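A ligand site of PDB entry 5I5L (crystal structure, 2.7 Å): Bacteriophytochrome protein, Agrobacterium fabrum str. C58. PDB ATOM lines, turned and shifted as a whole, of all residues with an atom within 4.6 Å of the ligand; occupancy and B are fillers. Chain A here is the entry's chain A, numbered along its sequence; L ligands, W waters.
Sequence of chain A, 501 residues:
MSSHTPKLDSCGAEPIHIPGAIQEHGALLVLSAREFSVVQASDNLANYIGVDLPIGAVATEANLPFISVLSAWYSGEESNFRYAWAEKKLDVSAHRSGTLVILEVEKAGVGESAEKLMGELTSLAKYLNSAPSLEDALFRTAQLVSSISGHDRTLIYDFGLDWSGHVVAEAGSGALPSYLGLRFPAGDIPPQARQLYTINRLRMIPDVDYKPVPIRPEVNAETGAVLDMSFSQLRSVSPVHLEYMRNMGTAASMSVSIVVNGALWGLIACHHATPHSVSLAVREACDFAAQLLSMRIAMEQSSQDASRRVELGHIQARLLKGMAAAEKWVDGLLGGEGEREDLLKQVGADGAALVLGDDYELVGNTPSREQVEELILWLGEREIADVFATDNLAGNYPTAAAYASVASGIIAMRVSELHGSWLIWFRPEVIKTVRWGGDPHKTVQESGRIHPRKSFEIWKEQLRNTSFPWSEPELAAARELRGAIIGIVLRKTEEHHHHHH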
ATOM      1  N   CYS A  11      25.184 -26.032  20.127  1.00  0.00           N
ATOM      2  CA  CYS A  11      24.746 -24.947  19.224  1.00  0.00           C
ATOM      3  C   CYS A  11      25.750 -23.803  19.107  1.00  0.00           C
ATOM      4  O   CYS A  11      26.163 -23.442  17.999  1.00  0.00           O
ATOM      5  CB  CYS A  11      23.383 -24.408  19.653  1.00  0.00           C
ATOM      6  SG  CYS A  11      22.536 -23.476  18.346  1.00  0.00           S
ATOM      7  N   ILE A  16      32.364 -19.730  14.049  1.00  0.00           N
ATOM      8  CA  ILE A  16      31.954 -19.129  12.784  1.00  0.00           C
ATOM      9  C   ILE A  16      32.983 -18.187  12.166  1.00  0.00           C
ATOM     10  O   ILE A  16      32.878 -17.849  11.007  1.00  0.00           O
ATOM     11  CB  ILE A  16      30.610 -18.386  12.915  1.00  0.00           C
ATOM     12  CG1 ILE A  16      30.776 -17.057  13.675  1.00  0.00           C
ATOM     13  CG2 ILE A  16      29.571 -19.306  13.554  1.00  0.00           C
ATOM     14  CD1 ILE A  16      29.487 -16.436  14.151  1.00  0.00           C
ATOM     15  N   LEU A 155      13.660  -5.198   8.349  1.00  0.00           N
ATOM     16  CA  LEU A 155      13.026  -5.167   9.676  1.00  0.00           C
ATOM     17  C   LEU A 155      14.013  -4.861  10.760  1.00  0.00           C
ATOM     18  O   LEU A 155      15.206  -5.030  10.581  1.00  0.00           O
ATOM     19  CB  LEU A 155      12.265  -6.465   9.977  1.00  0.00           C
ATOM     20  CG  LEU A 155      13.006  -7.807  10.049  1.00  0.00           C
ATOM     21  CD1 LEU A 155      13.693  -7.996  11.400  1.00  0.00           C
ATOM     22  CD2 LEU A 155      12.056  -8.967   9.793  1.00  0.00           C
ATOM     23  N   TYR A 157      14.919  -5.802  14.681  1.00  0.00           N
ATOM     24  CA  TYR A 157      14.745  -6.929  15.579  1.00  0.00           C
ATOM     25  C   TYR A 157      15.358  -6.550  16.911  1.00  0.00           C
ATOM     26  O   TYR A 157      16.557  -6.356  16.986  1.00  0.00           O
ATOM     27  CB  TYR A 157      15.464  -8.142  14.967  1.00  0.00           C
ATOM     28  CG  TYR A 157      15.337  -9.455  15.708  1.00  0.00           C
ATOM     29  CD1 TYR A 157      14.159 -10.214  15.663  1.00  0.00           C
ATOM     30  CD2 TYR A 157      16.402  -9.982  16.403  1.00  0.00           C
ATOM     31  CE1 TYR A 157      14.070 -11.440  16.313  1.00  0.00           C
ATOM     32  CE2 TYR A 157      16.322 -11.197  17.071  1.00  0.00           C
ATOM     33  CZ  TYR A 157      15.159 -11.931  17.030  1.00  0.00           C
ATOM     34  OH  TYR A 157      15.111 -13.139  17.704  1.00  0.00           O
ATOM     35  N   VAL A 167      10.243  -8.457  16.428  1.00  0.00           N
ATOM     36  CA  VAL A 167      10.338  -7.521  15.326  1.00  0.00           C
ATOM     37  C   VAL A 167       9.530  -6.315  15.733  1.00  0.00           C
ATOM     38  O   VAL A 167       8.367  -6.458  16.092  1.00  0.00           O
ATOM     39  CB  VAL A 167       9.786  -8.111  14.018  1.00  0.00           C
ATOM     40  CG1 VAL A 167       9.926  -7.108  12.870  1.00  0.00           C
ATOM     41  CG2 VAL A 167      10.497  -9.418  13.674  1.00  0.00           C
ATOM     42  N   TYR A 179       6.697 -10.210   9.197  1.00  0.00           N
ATOM     43  CA  TYR A 179       6.941 -10.690  10.558  1.00  0.00           C
ATOM     44  C   TYR A 179       6.745  -9.647  11.682  1.00  0.00           C
ATOM     45  O   TYR A 179       7.038  -9.932  12.844  1.00  0.00           O
ATOM     46  CB  TYR A 179       8.362 -11.266  10.665  1.00  0.00           C
ATOM     47  CG  TYR A 179       8.652 -12.467   9.797  1.00  0.00           C
ATOM     48  CD1 TYR A 179       7.698 -13.470   9.590  1.00  0.00           C
ATOM     49  CD2 TYR A 179       9.911 -12.629   9.212  1.00  0.00           C
ATOM     50  CE1 TYR A 179       7.975 -14.567   8.804  1.00  0.00           C
ATOM     51  CE2 TYR A 179      10.195 -13.742   8.426  1.00  0.00           C
ATOM     52  CZ  TYR A 179       9.230 -14.700   8.220  1.00  0.00           C
ATOM     53  OH  TYR A 179       9.508 -15.796   7.433  1.00  0.00           O
ATOM     54  N   PHE A 184      11.043 -14.334  18.146  1.00  0.00           N
ATOM     55  CA  PHE A 184      11.817 -15.451  17.636  1.00  0.00           C
ATOM     56  C   PHE A 184      12.708 -15.891  18.763  1.00  0.00           C
ATOM     57  O   PHE A 184      13.155 -15.051  19.535  1.00  0.00           O
ATOM     58  CB  PHE A 184      12.678 -15.027  16.437  1.00  0.00           C
ATOM     59  CG  PHE A 184      11.917 -14.871  15.157  1.00  0.00           C
ATOM     60  CD1 PHE A 184      11.192 -13.699  14.901  1.00  0.00           C
ATOM     61  CD2 PHE A 184      11.950 -15.869  14.183  1.00  0.00           C
ATOM     62  CE1 PHE A 184      10.485 -13.555  13.710  1.00  0.00           C
ATOM     63  CE2 PHE A 184      11.255 -15.727  12.980  1.00  0.00           C
ATOM     64  CZ  PHE A 184      10.525 -14.563  12.744  1.00  0.00           C
ATOM     65  N   GLY A 187      17.974 -19.161  20.098  1.00  0.00           N
ATOM     66  CA  GLY A 187      18.867 -20.037  19.361  1.00  0.00           C
ATOM     67  C   GLY A 187      18.992 -19.722  17.885  1.00  0.00           C
ATOM     68  O   GLY A 187      19.900 -20.252  17.217  1.00  0.00           O
ATOM     69  N   ASP A 188      18.065 -18.912  17.365  1.00  0.00           N
ATOM     70  CA  ASP A 188      18.131 -18.418  15.986  1.00  0.00           C
ATOM     71  C   ASP A 188      19.373 -17.594  15.708  1.00  0.00           C
ATOM     72  O   ASP A 188      19.857 -17.567  14.584  1.00  0.00           O
ATOM     73  CB  ASP A 188      16.880 -17.611  15.634  1.00  0.00           C
ATOM     74  CG  ASP A 188      15.643 -18.471  15.386  1.00  0.00           C
ATOM     75  OD1 ASP A 188      15.655 -19.694  15.660  1.00  0.00           O
ATOM     76  OD2 ASP A 188      14.657 -17.911  14.873  1.00  0.00           O
ATOM     77  N   ILE A 189      19.866 -16.895  16.735  1.00  0.00           N
ATOM     78  CA  ILE A 189      21.132 -16.173  16.651  1.00  0.00           C
ATOM     79  C   ILE A 189      21.927 -16.535  17.885  1.00  0.00           C
ATOM     80  O   ILE A 189      21.872 -15.839  18.885  1.00  0.00           O
ATOM     81  CB  ILE A 189      20.916 -14.646  16.567  1.00  0.00           C
ATOM     82  CG1 ILE A 189      19.896 -14.334  15.474  1.00  0.00           C
ATOM     83  CG2 ILE A 189      22.240 -13.937  16.321  1.00  0.00           C
ATOM     84  CD1 ILE A 189      19.789 -12.872  15.112  1.00  0.00           C
ATOM     85  N   PRO A 190      22.685 -17.643  17.819  1.00  0.00           N
ATOM     86  CA  PRO A 190      23.357 -18.151  19.023  1.00  0.00           C
ATOM     87  C   PRO A 190      24.478 -17.230  19.525  1.00  0.00           C
ATOM     88  O   PRO A 190      24.834 -16.276  18.843  1.00  0.00           O
ATOM     89  CB  PRO A 190      23.907 -19.516  18.574  1.00  0.00           C
ATOM     90  CG  PRO A 190      24.102 -19.366  17.082  1.00  0.00           C
ATOM     91  CD  PRO A 190      23.062 -18.383  16.599  1.00  0.00           C
ATOM     92  N   ALA A 193      27.591 -15.964  17.509  1.00  0.00           N
ATOM     93  CA  ALA A 193      27.128 -15.057  16.456  1.00  0.00           C
ATOM     94  C   ALA A 193      26.828 -13.667  16.999  1.00  0.00           C
ATOM     95  O   ALA A 193      27.283 -12.673  16.452  1.00  0.00           O
ATOM     96  CB  ALA A 193      25.906 -15.621  15.763  1.00  0.00           C
ATOM     97  N   TYR A 197      28.737 -10.178  16.207  1.00  0.00           N
ATOM     98  CA  TYR A 197      27.980  -9.088  15.624  1.00  0.00           C
ATOM     99  C   TYR A 197      28.052  -7.832  16.464  1.00  0.00           C
ATOM    100  O   TYR A 197      27.698  -6.771  15.979  1.00  0.00           O
ATOM    101  CB  TYR A 197      26.517  -9.479  15.381  1.00  0.00           C
ATOM    102  CG  TYR A 197      26.324 -10.687  14.463  1.00  0.00           C
ATOM    103  CD1 TYR A 197      27.339 -11.154  13.630  1.00  0.00           C
ATOM    104  CD2 TYR A 197      25.107 -11.361  14.450  1.00  0.00           C
ATOM    105  CE1 TYR A 197      27.163 -12.252  12.814  1.00  0.00           C
ATOM    106  CE2 TYR A 197      24.919 -12.464  13.638  1.00  0.00           C
ATOM    107  CZ  TYR A 197      25.950 -12.899  12.817  1.00  0.00           C
ATOM    108  OH  TYR A 197      25.809 -13.995  11.985  1.00  0.00           O
ATOM    109  N   ARG A 203      26.960  -7.467   7.905  1.00  0.00           N
ATOM    110  CA  ARG A 203      27.113  -8.738   7.180  1.00  0.00           C
ATOM    111  C   ARG A 203      26.162  -8.850   6.032  1.00  0.00           C
ATOM    112  O   ARG A 203      25.060  -8.335   6.093  1.00  0.00           O
ATOM    113  CB  ARG A 203      26.947  -9.935   8.113  1.00  0.00           C
ATOM    114  CG  ARG A 203      25.585 -10.011   8.790  1.00  0.00           C
ATOM    115  CD  ARG A 203      25.733 -10.548  10.201  1.00  0.00           C
ATOM    116  NE  ARG A 203      26.413  -9.577  11.067  1.00  0.00           N
ATOM    117  CZ  ARG A 203      25.853  -8.518  11.639  1.00  0.00           C
ATOM    118  NH1 ARG A 203      26.586  -7.723  12.392  1.00  0.00           N
ATOM    119  NH2 ARG A 203      24.551  -8.245  11.463  1.00  0.00           N
ATOM    120  N   ILE A 205      24.950 -11.664   2.749  1.00  0.00           N
ATOM    121  CA  ILE A 205      24.909 -12.984   2.165  1.00  0.00           C
ATOM    122  C   ILE A 205      24.105 -12.841   0.883  1.00  0.00           C
ATOM    123  O   ILE A 205      22.890 -13.038   0.891  1.00  0.00           O
ATOM    124  CB  ILE A 205      24.228 -14.007   3.114  1.00  0.00           C
ATOM    125  CG1 ILE A 205      24.867 -14.002   4.521  1.00  0.00           C
ATOM    126  CG2 ILE A 205      24.310 -15.427   2.535  1.00  0.00           C
ATOM    127  CD1 ILE A 205      24.179 -14.906   5.538  1.00  0.00           C
ATOM    128  N   ARG A 235      33.417 -13.298   4.494  1.00  0.00           N
ATOM    129  CA  ARG A 235      33.513 -14.582   5.193  1.00  0.00           C
ATOM    130  C   ARG A 235      32.377 -15.524   4.802  1.00  0.00           C
ATOM    131  O   ARG A 235      31.233 -15.102   4.692  1.00  0.00           O
ATOM    132  CB  ARG A 235      33.461 -14.329   6.701  1.00  0.00           C
ATOM    133  CG  ARG A 235      33.534 -15.579   7.569  1.00  0.00           C
ATOM    134  CD  ARG A 235      33.567 -15.210   9.041  1.00  0.00           C
ATOM    135  NE  ARG A 235      32.364 -14.475   9.416  1.00  0.00           N
ATOM    136  CZ  ARG A 235      31.173 -15.010   9.666  1.00  0.00           C
ATOM    137  NH1 ARG A 235      30.976 -16.326   9.600  1.00  0.00           N
ATOM    138  NH2 ARG A 235      30.151 -14.228   9.970  1.00  0.00           N
ATOM    139  N   VAL A 237      29.586 -17.946   5.606  1.00  0.00           N
ATOM    140  CA  VAL A 237      28.717 -18.119   6.770  1.00  0.00           C
ATOM    141  C   VAL A 237      28.470 -19.578   7.135  1.00  0.00           C
ATOM    142  O   VAL A 237      28.725 -20.495   6.353  1.00  0.00           O
ATOM    143  CB  VAL A 237      27.350 -17.397   6.601  1.00  0.00           C
ATOM    144  CG1 VAL A 237      27.566 -15.920   6.260  1.00  0.00           C
ATOM    145  CG2 VAL A 237      26.461 -18.092   5.577  1.00  0.00           C
ATOM    146  N   SER A 238      27.946 -19.762   8.331  1.00  0.00           N
ATOM    147  CA  SER A 238      27.610 -21.070   8.858  1.00  0.00           C
ATOM    148  C   SER A 238      26.631 -21.835   7.950  1.00  0.00           C
ATOM    149  O   SER A 238      25.578 -21.310   7.589  1.00  0.00           O
ATOM    150  CB  SER A 238      26.957 -20.915  10.223  1.00  0.00           C
ATOM    151  OG  SER A 238      26.584 -22.176  10.724  1.00  0.00           O
ATOM    152  N   VAL A 240      24.568 -24.165   8.820  1.00  0.00           N
ATOM    153  CA  VAL A 240      23.287 -24.333   9.508  1.00  0.00           C
ATOM    154  C   VAL A 240      22.393 -23.090   9.352  1.00  0.00           C
ATOM    155  O   VAL A 240      21.183 -23.224   9.133  1.00  0.00           O
ATOM    156  CB  VAL A 240      23.446 -24.768  10.991  1.00  0.00           C
ATOM    157  CG1 VAL A 240      24.178 -23.757  11.847  1.00  0.00           C
ATOM    158  CG2 VAL A 240      22.105 -25.070  11.612  1.00  0.00           C
ATOM    159  N   HIS A 241      22.979 -21.900   9.416  1.00  0.00           N
ATOM    160  CA  HIS A 241      22.218 -20.692   9.169  1.00  0.00           C
ATOM    161  C   HIS A 241      21.660 -20.640   7.737  1.00  0.00           C
ATOM    162  O   HIS A 241      20.537 -20.156   7.533  1.00  0.00           O
ATOM    163  CB  HIS A 241      23.028 -19.415   9.432  1.00  0.00           C
ATOM    164  CG  HIS A 241      22.267 -18.173   9.114  1.00  0.00           C
ATOM    165  ND1 HIS A 241      20.998 -17.949   9.606  1.00  0.00           N
ATOM    166  CD2 HIS A 241      22.551 -17.135   8.306  1.00  0.00           C
ATOM    167  CE1 HIS A 241      20.547 -16.809   9.120  1.00  0.00           C
ATOM    168  NE2 HIS A 241      21.468 -16.294   8.333  1.00  0.00           N
ATOM    169  N   TYR A 244      18.528 -22.317   7.641  1.00  0.00           N
ATOM    170  CA  TYR A 244      17.542 -21.367   8.183  1.00  0.00           C
ATOM    171  C   TYR A 244      17.033 -20.431   7.079  1.00  0.00           C
ATOM    172  O   TYR A 244      15.832 -20.241   6.933  1.00  0.00           O
ATOM    173  CB  TYR A 244      18.152 -20.565   9.330  1.00  0.00           C
ATOM    174  CG  TYR A 244      17.227 -19.645  10.070  1.00  0.00           C
ATOM    175  CD1 TYR A 244      16.954 -18.356   9.597  1.00  0.00           C
ATOM    176  CD2 TYR A 244      16.686 -20.011  11.305  1.00  0.00           C
ATOM    177  CE1 TYR A 244      16.137 -17.493  10.304  1.00  0.00           C
ATOM    178  CE2 TYR A 244      15.869 -19.141  12.020  1.00  0.00           C
ATOM    179  CZ  TYR A 244      15.593 -17.886  11.523  1.00  0.00           C
ATOM    180  OH  TYR A 244      14.779 -17.039  12.245  1.00  0.00           O
ATOM    181  N   MET A 245      17.943 -19.871   6.292  1.00  0.00           N
ATOM    182  CA  MET A 245      17.534 -19.007   5.183  1.00  0.00           C
ATOM    183  C   MET A 245      16.666 -19.718   4.133  1.00  0.00           C
ATOM    184  O   MET A 245      15.660 -19.158   3.673  1.00  0.00           O
ATOM    185  CB  MET A 245      18.754 -18.350   4.532  1.00  0.00           C
ATOM    186  CG  MET A 245      19.328 -17.224   5.370  1.00  0.00           C
ATOM    187  SD  MET A 245      20.908 -16.667   4.734  1.00  0.00           S
ATOM    188  CE  MET A 245      20.394 -15.752   3.289  1.00  0.00           C
ATOM    189  N   MET A 248      13.365 -20.469   5.608  1.00  0.00           N
ATOM    190  CA  MET A 248      12.595 -19.220   5.578  1.00  0.00           C
ATOM    191  C   MET A 248      12.183 -18.793   4.161  1.00  0.00           C
ATOM    192  O   MET A 248      11.174 -18.111   3.980  1.00  0.00           O
ATOM    193  CB  MET A 248      13.395 -18.106   6.250  1.00  0.00           C
ATOM    194  CG  MET A 248      12.590 -16.858   6.580  1.00  0.00           C
ATOM    195  SD  MET A 248      13.479 -15.772   7.700  1.00  0.00           S
ATOM    196  CE  MET A 248      12.954 -16.431   9.271  1.00  0.00           C
ATOM    197  N   SER A 253      20.294 -12.216   2.146  1.00  0.00           N
ATOM    198  CA  SER A 253      20.104 -11.460   3.389  1.00  0.00           C
ATOM    199  C   SER A 253      21.206 -10.414   3.583  1.00  0.00           C
ATOM    200  O   SER A 253      22.230 -10.416   2.888  1.00  0.00           O
ATOM    201  CB  SER A 253      20.028 -12.403   4.603  1.00  0.00           C
ATOM    202  OG  SER A 253      21.314 -12.758   5.104  1.00  0.00           O
ATOM    203  N   MET A 254      20.952  -9.509   4.510  1.00  0.00           N
ATOM    204  CA  MET A 254      21.928  -8.490   4.902  1.00  0.00           C
ATOM    205  C   MET A 254      21.495  -7.937   6.247  1.00  0.00           C
ATOM    206  O   MET A 254      20.332  -7.563   6.406  1.00  0.00           O
ATOM    207  CB  MET A 254      21.982  -7.362   3.872  1.00  0.00           C
ATOM    208  CG  MET A 254      23.211  -6.490   4.004  1.00  0.00           C
ATOM    209  SD  MET A 254      22.996  -4.815   3.364  1.00  0.00           S
ATOM    210  CE  MET A 254      21.947  -4.095   4.640  1.00  0.00           C
ATOM    211  N   SER A 255      22.400  -7.895   7.218  1.00  0.00           N
ATOM    212  CA  SER A 255      22.052  -7.365   8.528  1.00  0.00           C
ATOM    213  C   SER A 255      23.130  -6.447   9.087  1.00  0.00           C
ATOM    214  O   SER A 255      24.306  -6.530   8.713  1.00  0.00           O
ATOM    215  CB  SER A 255      21.706  -8.485   9.516  1.00  0.00           C
ATOM    216  OG  SER A 255      22.728  -9.465   9.586  1.00  0.00           O
ATOM    217  N   LEU A 267      18.990  -5.738  15.589  1.00  0.00           N
ATOM    218  CA  LEU A 267      19.502  -5.839  14.206  1.00  0.00           C
ATOM    219  C   LEU A 267      18.569  -5.123  13.263  1.00  0.00           C
ATOM    220  O   LEU A 267      17.363  -5.148  13.438  1.00  0.00           O
ATOM    221  CB  LEU A 267      19.583  -7.299  13.755  1.00  0.00           C
ATOM    222  CG  LEU A 267      20.574  -8.251  14.425  1.00  0.00           C
ATOM    223  CD1 LEU A 267      20.421  -9.643  13.853  1.00  0.00           C
ATOM    224  CD2 LEU A 267      22.022  -7.770  14.244  1.00  0.00           C
ATOM    225  N   HIS A 271      16.127  -8.906   3.895  1.00  0.00           N
ATOM    226  CA  HIS A 271      16.048 -10.162   3.148  1.00  0.00           C
ATOM    227  C   HIS A 271      15.401  -9.937   1.792  1.00  0.00           C
ATOM    228  O   HIS A 271      14.474  -9.131   1.662  1.00  0.00           O
ATOM    229  CB  HIS A 271      15.212 -11.193   3.908  1.00  0.00           C
ATOM    230  CG  HIS A 271      15.703 -11.488   5.288  1.00  0.00           C
ATOM    231  ND1 HIS A 271      16.625 -12.471   5.561  1.00  0.00           N
ATOM    232  CD2 HIS A 271      15.369 -10.944   6.479  1.00  0.00           C
ATOM    233  CE1 HIS A 271      16.855 -12.515   6.859  1.00  0.00           C
ATOM    234  NE2 HIS A 271      16.105 -11.597   7.438  1.00  0.00           N
ATOM    235  N   ILE A 450      21.994 -30.013  15.761  1.00  0.00           N
ATOM    236  CA  ILE A 450      20.689 -29.343  15.875  1.00  0.00           C
ATOM    237  C   ILE A 450      20.442 -28.543  14.593  1.00  0.00           C
ATOM    238  O   ILE A 450      21.220 -27.645  14.271  1.00  0.00           O
ATOM    239  CB  ILE A 450      20.609 -28.406  17.090  1.00  0.00           C
ATOM    240  N   HIS A 451      19.383 -28.891  13.853  1.00  0.00           N
ATOM    241  CA  HIS A 451      19.019 -28.220  12.593  1.00  0.00           C
ATOM    242  C   HIS A 451      17.834 -27.269  12.859  1.00  0.00           C
ATOM    243  O   HIS A 451      17.094 -27.446  13.825  1.00  0.00           O
ATOM    244  CB  HIS A 451      18.608 -29.237  11.511  1.00  0.00           C
ATOM    245  CG  HIS A 451      19.742 -29.986  10.870  1.00  0.00           C
ATOM    246  ND1 HIS A 451      21.026 -30.015  11.392  1.00  0.00           N
ATOM    247  CD2 HIS A 451      19.763 -30.775   9.766  1.00  0.00           C
ATOM    248  CE1 HIS A 451      21.788 -30.766  10.613  1.00  0.00           C
ATOM    249  NE2 HIS A 451      21.048 -31.242   9.620  1.00  0.00           N
ATOM    250  N   PRO A 452      17.654 -26.263  11.980  1.00  0.00           N
ATOM    251  CA  PRO A 452      16.551 -25.301  12.154  1.00  0.00           C
ATOM    252  C   PRO A 452      15.186 -25.844  11.750  1.00  0.00           C
ATOM    253  O   PRO A 452      15.083 -26.628  10.817  1.00  0.00           O
ATOM    254  CB  PRO A 452      16.949 -24.132  11.229  1.00  0.00           C
ATOM    255  CG  PRO A 452      17.850 -24.741  10.217  1.00  0.00           C
ATOM    256  CD  PRO A 452      18.573 -25.854  10.900  1.00  0.00           C
HETATM  257  C1  LIG L   1      22.775 -16.020  11.886  1.00  0.00           C
HETATM  258  N1  LIG L   1      20.367 -15.814  12.308  1.00  0.00           N
HETATM  259  C2  LIG L   1      21.568 -15.356  11.911  1.00  0.00           C
HETATM  260  C3  LIG L   1      21.442 -14.087  11.466  1.00  0.00           C
HETATM  261  C4  LIG L   1      20.177 -13.718  11.604  1.00  0.00           C
HETATM  262  C5  LIG L   1      19.516 -14.786  12.100  1.00  0.00           C
HETATM  263  C6  LIG L   1      19.638 -12.323  11.242  1.00  0.00           C
HETATM  264  C7  LIG L   1      22.552 -13.160  10.899  1.00  0.00           C
HETATM  265  C8  LIG L   1      22.844 -13.364   9.397  1.00  0.00           C
HETATM  266  C9  LIG L   1      21.771 -12.736   8.481  1.00  0.00           C
HETATM  267  O1  LIG L   1      21.830 -11.495   8.243  1.00  0.00           O
HETATM  268  O2  LIG L   1      20.920 -13.514   7.994  1.00  0.00           O
HETATM  269  C10 LIG L   1      18.211 -14.914  12.462  1.00  0.00           C
HETATM  270  N2  LIG L   1      16.931 -13.982  10.617  1.00  0.00           N
HETATM  271  C11 LIG L   1      17.125 -14.328  11.901  1.00  0.00           C
HETATM  272  C12 LIG L   1      16.018 -14.065  12.635  1.00  0.00           C
HETATM  273  C13 LIG L   1      15.118 -13.512  11.821  1.00  0.00           C
HETATM  274  C14 LIG L   1      15.691 -13.483  10.614  1.00  0.00           C
HETATM  275  C15 LIG L   1      15.769 -14.313  14.133  1.00  0.00           C
HETATM  276  O3  LIG L   1      15.134 -13.038   9.609  1.00  0.00           O
HETATM  277  C16 LIG L   1      13.872 -13.122  12.166  1.00  0.00           C
HETATM  278  C17 LIG L   1      13.316 -11.980  11.746  1.00  0.00           C
HETATM  279  N3  LIG L   1      20.342 -20.461  13.761  1.00  0.00           N
HETATM  280  C18 LIG L   1      19.466 -21.405  14.113  1.00  0.00           C
HETATM  281  C19 LIG L   1      20.045 -22.485  14.597  1.00  0.00           C
HETATM  282  C20 LIG L   1      21.353 -22.263  14.564  1.00  0.00           C
HETATM  283  C21 LIG L   1      21.539 -21.017  14.041  1.00  0.00           C
HETATM  284  C22 LIG L   1      19.318 -23.756  15.086  1.00  0.00           C
HETATM  285  O4  LIG L   1      18.242 -21.322  14.009  1.00  0.00           O
HETATM  286  C23 LIG L   1      22.393 -23.302  15.031  1.00  0.00           C
HETATM  287  C24 LIG L   1      22.327 -23.511  16.545  1.00  0.00           C
HETATM  288  C25 LIG L   1      22.770 -20.469  13.871  1.00  0.00           C
HETATM  289  N4  LIG L   1      22.309 -18.227  12.898  1.00  0.00           N
HETATM  290  C26 LIG L   1      23.084 -19.267  13.277  1.00  0.00           C
HETATM  291  C27 LIG L   1      24.360 -18.903  13.029  1.00  0.00           C
HETATM  292  C28 LIG L   1      24.372 -17.686  12.507  1.00  0.00           C
HETATM  293  C29 LIG L   1      23.105 -17.239  12.417  1.00  0.00           C
HETATM  294  C30 LIG L   1      25.605 -19.759  13.291  1.00  0.00           C
HETATM  295  C31 LIG L   1      25.497 -17.053  12.118  1.00  0.00           C
HETATM  296  C32 LIG L   1      25.919 -17.090  10.626  1.00  0.00           C
HETATM  297  C33 LIG L   1      27.318 -16.506  10.382  1.00  0.00           C
HETATM  298  O5  LIG L   1      27.472 -15.289  10.616  1.00  0.00           O
HETATM  299  O6  LIG L   1      28.196 -17.266   9.929  1.00  0.00           O
HETATM  300  O   HOH W   1      19.618 -18.741  11.748  1.00  0.00           O
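An oxygen (O2) of the ligand lies within hydrogen-bond range of a ring nitrogen (NE2) of His 241 (2.9 Å). O3 of the ligand sits at hydrogen-bond distance from NE2 of His 271, 2.8 Å away. OH of Tyr 197 is in hydrogen-bond range of O5 of the ligand (2.5 Å). An oxygen (O6) of the ligand sits at hydrogen-bond distance from the backbone NH of Ser 238 (3.0 Å). N3 of the ligand sits close to O of Gly 187. O of Asp 188 is in hydrogen-bond range of N1 of the ligand (2.9 Å). The guanidinium group (NH2) of Arg 235 is in salt-bridge range of an oxygen (O5) of the ligand (3.0 Å). OG of Ser 255 sits at hydrogen-bond distance from O1 of the ligand, at 2.6 Å. The side-chain sulfur (SG) of Cys 11 is covalently linked to a carbon (C24) of the ligand, 1.8 Å away. The side-chain hydroxyl (OG) of Ser 253 sits at hydrogen-bond distance from an oxygen (O2) of the ligand (3.0 Å).
NH1 of Arg 235 lies within hydrogen-bond range of O of Ile 16 (2.8 Å). The backbone NH (N) of Tyr 157 lies within hydrogen-bond range of the backbone carbonyl oxygen (O) of Leu 267, at 2.8 Å. The side-chain hydroxyl of Ser 238 lies close to the backbone NH of Val 240 (3.4 Å). OD2 of Asp 188 lies within hydrogen-bond range of OH of Tyr 244 (2.8 Å). The side-chain hydroxyl of Tyr 157 is in hydrogen-bond range of the backbone carbonyl oxygen of Phe 184, 3.3 Å away. A ring nitrogen (NE2) of His 241 is in hydrogen-bond range of the side-chain sulfur (SD) of Met 245, 3.7 Å away. N of Ile 205 sits at hydrogen-bond distance from O of Ser 253 (3.0 Å). OG of Ser 255 sits at hydrogen-bond distance from NH2 of Arg 203, 2.9 Å away.
SD of Met 248 sits close to O3 of the ligand (3.7 Å). Merely in contact with the ligand: Ile 16, Leu 155, Tyr 157, Phe 184, Ile 189, Pro 190, Ala 193, Val 237, Val 240, Tyr 244 and Leu 267. Hydrophobic or aromatic side chains that line the ligand: Ile 16, Leu 155, Tyr 157, Phe 184, Ile 189, Pro 190, Ala 193, Tyr 197, Val 237, Val 240, His 241, Tyr 244, Met 248, Leu 267 and His 271. Of the 31 residues printed, 22 come within 4 Å of the ligand. The nearest printed residue that does not touch the ligand is Arg 203 (4.1 Å).
Water W1 lies within hydrogen-bond range of ND1 of His 241, N3 of the ligand and O of Asp 188.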
